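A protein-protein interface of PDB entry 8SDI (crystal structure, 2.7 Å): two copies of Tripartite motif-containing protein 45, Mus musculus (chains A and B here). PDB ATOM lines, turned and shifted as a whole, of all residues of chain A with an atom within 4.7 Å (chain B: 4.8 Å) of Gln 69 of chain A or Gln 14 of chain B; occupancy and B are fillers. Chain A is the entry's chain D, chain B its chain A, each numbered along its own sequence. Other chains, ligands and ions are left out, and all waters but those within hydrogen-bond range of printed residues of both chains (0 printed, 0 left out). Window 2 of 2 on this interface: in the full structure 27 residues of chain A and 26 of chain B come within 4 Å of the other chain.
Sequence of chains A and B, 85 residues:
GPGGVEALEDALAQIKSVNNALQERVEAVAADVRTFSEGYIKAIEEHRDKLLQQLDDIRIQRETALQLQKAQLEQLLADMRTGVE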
ATOM      1  N   ALA A  65      23.608 -12.330   9.690  1.00  0.00           N
ATOM      2  CA  ALA A  65      23.682 -13.765   9.456  1.00  0.00           C
ATOM      3  C   ALA A  65      23.637 -14.499  10.794  1.00  0.00           C
ATOM      4  O   ALA A  65      22.847 -15.425  10.948  1.00  0.00           O
ATOM      5  CB  ALA A  65      24.898 -14.127   8.655  1.00  0.00           C
ATOM      6  N   LEU A  66      24.442 -14.039  11.764  1.00  0.00           N
ATOM      7  CA  LEU A  66      24.479 -14.587  13.112  1.00  0.00           C
ATOM      8  C   LEU A  66      23.054 -14.754  13.630  1.00  0.00           C
ATOM      9  O   LEU A  66      22.614 -15.863  13.925  1.00  0.00           O
ATOM     10  CB  LEU A  66      25.285 -13.620  13.988  1.00  0.00           C
ATOM     11  CG  LEU A  66      25.117 -13.725  15.506  1.00  0.00           C
ATOM     12  CD1 LEU A  66      26.106 -14.729  16.079  1.00  0.00           C
ATOM     13  CD2 LEU A  66      25.361 -12.367  16.159  1.00  0.00           C
ATOM     14  N   GLN A  67      22.334 -13.636  13.736  1.00  0.00           N
ATOM     15  CA  GLN A  67      21.033 -13.626  14.370  1.00  0.00           C
ATOM     16  C   GLN A  67      20.096 -14.611  13.667  1.00  0.00           C
ATOM     17  O   GLN A  67      19.430 -15.385  14.336  1.00  0.00           O
ATOM     18  CB  GLN A  67      20.549 -12.181  14.477  1.00  0.00           C
ATOM     19  CG  GLN A  67      21.380 -11.336  15.434  1.00  0.00           C
ATOM     20  CD  GLN A  67      21.217 -11.711  16.891  1.00  0.00           C
ATOM     21  OE1 GLN A  67      20.213 -12.284  17.306  1.00  0.00           O
ATOM     22  NE2 GLN A  67      22.225 -11.401  17.690  1.00  0.00           N
ATOM     23  N   LEU A  68      20.070 -14.611  12.329  1.00  0.00           N
ATOM     24  CA  LEU A  68      19.253 -15.545  11.563  1.00  0.00           C
ATOM     25  C   LEU A  68      19.582 -16.987  11.938  1.00  0.00           C
ATOM     26  O   LEU A  68      18.698 -17.835  12.058  1.00  0.00           O
ATOM     27  CB  LEU A  68      19.549 -15.369  10.072  1.00  0.00           C
ATOM     28  CG  LEU A  68      18.479 -14.676   9.232  1.00  0.00           C
ATOM     29  CD1 LEU A  68      18.800 -14.813   7.749  1.00  0.00           C
ATOM     30  CD2 LEU A  68      17.092 -15.236   9.520  1.00  0.00           C
ATOM     31  N   GLN A  69      20.874 -17.282  12.067  1.00  0.00           N
ATOM     32  CA  GLN A  69      21.241 -18.614  12.494  1.00  0.00           C
ATOM     33  C   GLN A  69      20.689 -18.852  13.895  1.00  0.00           C
ATOM     34  O   GLN A  69      19.804 -19.689  14.057  1.00  0.00           O
ATOM     35  CB  GLN A  69      22.745 -18.829  12.363  1.00  0.00           C
ATOM     36  CG  GLN A  69      23.125 -19.352  10.987  1.00  0.00           C
ATOM     37  CD  GLN A  69      24.618 -19.328  10.780  1.00  0.00           C
ATOM     38  OE1 GLN A  69      25.385 -19.376  11.740  1.00  0.00           O
ATOM     39  NE2 GLN A  69      25.033 -19.245   9.522  1.00  0.00           N
ATOM     40  N   LYS A  70      21.176 -18.065  14.866  1.00  0.00           N
ATOM     41  CA  LYS A  70      20.817 -18.220  16.265  1.00  0.00           C
ATOM     42  C   LYS A  70      19.323 -18.492  16.370  1.00  0.00           C
ATOM     43  O   LYS A  70      18.884 -19.447  17.008  1.00  0.00           O
ATOM     44  CB  LYS A  70      21.174 -16.950  17.040  1.00  0.00           C
ATOM     45  CG  LYS A  70      20.843 -17.004  18.527  1.00  0.00           C
ATOM     46  CD  LYS A  70      21.312 -15.795  19.356  1.00  0.00           C
ATOM     47  CE  LYS A  70      22.599 -15.146  18.888  1.00  0.00           C
ATOM     48  NZ  LYS A  70      23.029 -14.071  19.815  1.00  0.00           N
ATOM     49  N   ALA A  71      18.553 -17.628  15.709  1.00  0.00           N
ATOM     50  CA  ALA A  71      17.108 -17.735  15.724  1.00  0.00           C
ATOM     51  C   ALA A  71      16.690 -19.041  15.068  1.00  0.00           C
ATOM     52  O   ALA A  71      15.851 -19.745  15.601  1.00  0.00           O
ATOM     53  CB  ALA A  71      16.466 -16.540  15.068  1.00  0.00           C
ATOM     54  N   GLN A  72      17.294 -19.393  13.937  1.00  0.00           N
ATOM     55  CA  GLN A  72      16.860 -20.632  13.316  1.00  0.00           C
ATOM     56  C   GLN A  72      17.197 -21.838  14.195  1.00  0.00           C
ATOM     57  O   GLN A  72      16.498 -22.849  14.177  1.00  0.00           O
ATOM     58  CB  GLN A  72      17.434 -20.784  11.919  1.00  0.00           C
ATOM     59  CG  GLN A  72      16.556 -21.707  11.093  1.00  0.00           C
ATOM     60  CD  GLN A  72      16.301 -21.140   9.721  1.00  0.00           C
ATOM     61  OE1 GLN A  72      16.758 -20.043   9.389  1.00  0.00           O
ATOM     62  NE2 GLN A  72      15.573 -21.897   8.912  1.00  0.00           N
ATOM     63  N   LEU A  73      18.263 -21.713  14.983  1.00  0.00           N
ATOM     64  CA  LEU A  73      18.698 -22.800  15.829  1.00  0.00           C
ATOM     65  C   LEU A  73      17.714 -22.956  16.979  1.00  0.00           C
ATOM     66  O   LEU A  73      17.334 -24.082  17.310  1.00  0.00           O
ATOM     67  CB  LEU A  73      20.094 -22.478  16.367  1.00  0.00           C
ATOM     68  CG  LEU A  73      21.283 -22.991  15.554  1.00  0.00           C
ATOM     69  CD1 LEU A  73      22.489 -23.218  16.453  1.00  0.00           C
ATOM     70  CD2 LEU A  73      20.947 -24.262  14.796  1.00  0.00           C
ATOM     71  N   ASP B  10      17.090 -26.705   6.328  1.00  0.00           N
ATOM     72  CA  ASP B  10      16.918 -25.321   5.917  1.00  0.00           C
ATOM     73  C   ASP B  10      18.089 -24.501   6.432  1.00  0.00           C
ATOM     74  O   ASP B  10      18.865 -23.939   5.657  1.00  0.00           O
ATOM     75  CB  ASP B  10      15.686 -24.684   6.556  1.00  0.00           C
ATOM     76  CG  ASP B  10      14.381 -25.202   5.992  1.00  0.00           C
ATOM     77  OD1 ASP B  10      14.407 -25.748   4.868  1.00  0.00           O
ATOM     78  OD2 ASP B  10      13.357 -25.061   6.687  1.00  0.00           O
ATOM     79  N   ALA B  11      18.156 -24.423   7.763  1.00  0.00           N
ATOM     80  CA  ALA B  11      19.239 -23.760   8.452  1.00  0.00           C
ATOM     81  C   ALA B  11      20.565 -24.172   7.818  1.00  0.00           C
ATOM     82  O   ALA B  11      21.475 -23.353   7.739  1.00  0.00           O
ATOM     83  CB  ALA B  11      19.180 -24.128   9.908  1.00  0.00           C
ATOM     84  N   LEU B  12      20.645 -25.424   7.338  1.00  0.00           N
ATOM     85  CA  LEU B  12      21.853 -25.929   6.699  1.00  0.00           C
ATOM     86  C   LEU B  12      22.034 -25.364   5.288  1.00  0.00           C
ATOM     87  O   LEU B  12      23.155 -25.073   4.889  1.00  0.00           O
ATOM     88  CB  LEU B  12      21.873 -27.461   6.703  1.00  0.00           C
ATOM     89  CG  LEU B  12      22.564 -28.119   7.903  1.00  0.00           C
ATOM     90  CD1 LEU B  12      22.142 -29.575   8.066  1.00  0.00           C
ATOM     91  CD2 LEU B  12      24.079 -28.022   7.794  1.00  0.00           C
ATOM     92  N   ALA B  13      20.947 -25.197   4.529  1.00  0.00           N
ATOM     93  CA  ALA B  13      21.073 -24.608   3.202  1.00  0.00           C
ATOM     94  C   ALA B  13      21.314 -23.100   3.288  1.00  0.00           C
ATOM     95  O   ALA B  13      22.009 -22.552   2.430  1.00  0.00           O
ATOM     96  CB  ALA B  13      19.885 -24.940   2.333  1.00  0.00           C
ATOM     97  N   GLN B  14      20.747 -22.444   4.319  1.00  0.00           N
ATOM     98  CA  GLN B  14      20.910 -21.014   4.549  1.00  0.00           C
ATOM     99  C   GLN B  14      22.376 -20.706   4.846  1.00  0.00           C
ATOM    100  O   GLN B  14      22.981 -19.837   4.220  1.00  0.00           O
ATOM    101  CB  GLN B  14      20.079 -20.561   5.750  1.00  0.00           C
ATOM    102  CG  GLN B  14      20.262 -19.089   6.101  1.00  0.00           C
ATOM    103  CD  GLN B  14      20.044 -18.809   7.567  1.00  0.00           C
ATOM    104  OE1 GLN B  14      19.039 -18.232   7.965  1.00  0.00           O
ATOM    105  NE2 GLN B  14      20.984 -19.230   8.397  1.00  0.00           N
ATOM    106  N   ILE B  15      22.924 -21.427   5.828  1.00  0.00           N
ATOM    107  CA  ILE B  15      24.321 -21.314   6.208  1.00  0.00           C
ATOM    108  C   ILE B  15      25.212 -21.350   4.968  1.00  0.00           C
ATOM    109  O   ILE B  15      26.057 -20.475   4.815  1.00  0.00           O
ATOM    110  CB  ILE B  15      24.690 -22.400   7.234  1.00  0.00           C
ATOM    111  CG1 ILE B  15      24.080 -22.057   8.595  1.00  0.00           C
ATOM    112  CG2 ILE B  15      26.197 -22.605   7.317  1.00  0.00           C
ATOM    113  CD1 ILE B  15      23.760 -23.253   9.451  1.00  0.00           C
ATOM    114  N   LYS B  16      25.004 -22.345   4.091  1.00  0.00           N
ATOM    115  CA  LYS B  16      25.810 -22.502   2.887  1.00  0.00           C
ATOM    116  C   LYS B  16      25.680 -21.292   1.962  1.00  0.00           C
ATOM    117  O   LYS B  16      26.597 -21.026   1.187  1.00  0.00           O
ATOM    118  CB  LYS B  16      25.481 -23.792   2.129  1.00  0.00           C
ATOM    119  CG  LYS B  16      26.127 -23.918   0.751  1.00  0.00           C
ATOM    120  CD  LYS B  16      25.893 -25.250   0.044  1.00  0.00           C
ATOM    121  CE  LYS B  16      26.024 -25.178  -1.466  1.00  0.00           C
ATOM    122  NZ  LYS B  16      24.842 -24.545  -2.110  1.00  0.00           N
ATOM    123  N   SER B  17      24.548 -20.576   2.040  1.00  0.00           N
ATOM    124  CA  SER B  17      24.292 -19.432   1.173  1.00  0.00           C
ATOM    125  C   SER B  17      24.644 -18.132   1.886  1.00  0.00           C
ATOM    126  O   SER B  17      25.192 -17.216   1.275  1.00  0.00           O
ATOM    127  CB  SER B  17      22.866 -19.383   0.729  1.00  0.00           C
ATOM    128  OG  SER B  17      22.076 -18.758   1.732  1.00  0.00           O
ATOM    129  N   VAL B  18      24.300 -18.042   3.172  1.00  0.00           N
ATOM    130  CA  VAL B  18      24.596 -16.810   3.872  1.00  0.00           C
ATOM    131  C   VAL B  18      26.113 -16.687   3.986  1.00  0.00           C
ATOM    132  O   VAL B  18      26.644 -15.585   4.122  1.00  0.00           O
ATOM    133  CB  VAL B  18      23.851 -16.726   5.212  1.00  0.00           C
ATOM    134  CG1 VAL B  18      24.544 -17.518   6.309  1.00  0.00           C
ATOM    135  CG2 VAL B  18      23.600 -15.281   5.608  1.00  0.00           C
ATOM    136  N   ASN B  19      26.801 -17.829   3.844  1.00  0.00           N
ATOM    137  CA  ASN B  19      28.256 -17.837   3.773  1.00  0.00           C
ATOM    138  C   ASN B  19      28.716 -17.408   2.378  1.00  0.00           C
ATOM    139  O   ASN B  19      29.593 -16.553   2.259  1.00  0.00           O
ATOM    140  CB  ASN B  19      28.896 -19.124   4.317  1.00  0.00           C
ATOM    141  CG  ASN B  19      29.015 -19.153   5.834  1.00  0.00           C
ATOM    142  OD1 ASN B  19      30.116 -19.126   6.376  1.00  0.00           O
ATOM    143  ND2 ASN B  19      27.899 -19.213   6.545  1.00  0.00           N
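No position is printed for both chains. Of the 8 pairs that touch across the chains among the printed residues, none has its exchanged pair printed and touching as well.
Of the 10 printed residues of chain B, 5 touch a printed residue of chain A. Printed residues of chain B that touch a printed residue of chain A: Asp 10, Ala 11, Gln 14, Ile 15 and Val 18. Hydrophobic or aromatic side chains of chain B that line the printed part of chain A: Ala 11, Ile 15 and Val 18. Of the 9 printed residues of chain A, 4 touch a printed residue of chain B. Hydrophobic or aromatic side chains of chain A within 4 Å of the printed part of chain B: Ala 65 and Leu 68. Along chain A the printed residues that touch a printed residue of chain B span positions 65 to 72.
Among the printed residues, pairs that only touch across the chains: Ala 65 of chain A with Val 18 of chain B (3.5 Å), Leu 68 of chain A with Gln 14 of chain B (3.4 Å), Gln 69 of chain A with Gln 14 of chain B (3.4 Å), Gln 69 of chain A with Ile 15 of chain B (3.1 Å), Gln 69 of chain A with Val 18 of chain B (3.7 Å), Gln 72 of chain A with Asp 10 of chain B (3.7 Å) and Gln 72 of chain A with Ala 11 of chain B (3.8 Å).
Of chain B, only Gln 14 (3.4 Å), Ile 15 (3.1 Å) and Val 18 (3.7 Å) come within 4 Å of Gln 69 of chain A. Of chain A, only Leu 68 (3.4 Å), Gln 69 (3.4 Å) and Gln 72 (3.2 Å) come within 4 Å of Gln 14 of chain B. Of the printed residues of chain A, Asp 10 of chain B touches Gln 72. Of the printed residues of chain A, Ile 15 of chain B touches Gln 69 (3.1 Å). Printed residues of chain B within 4 Å of Leu 68 of chain A: Gln 14. Printed residues of chain A within 4 Å of Val 18 of chain B: Ala 65 and Gln 69. Lys 16 of chain B touches none of the printed residues of chain A. Gln 67 of chain A touches none of the printed residues of chain B.
The side-chain amide oxygen (OE1) of Gln 14 of chain B sits close to the side-chain amide oxygen (OE1) of Gln 72 of chain A.
ND2 of Asn 19 of chain B is in hydrogen-bond range of O of Ile 15 of chain B (2.8 Å). O of Gln 14 of chain B sits at hydrogen-bond distance from OG of Ser 17 of chain B, 2.9 Å away.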
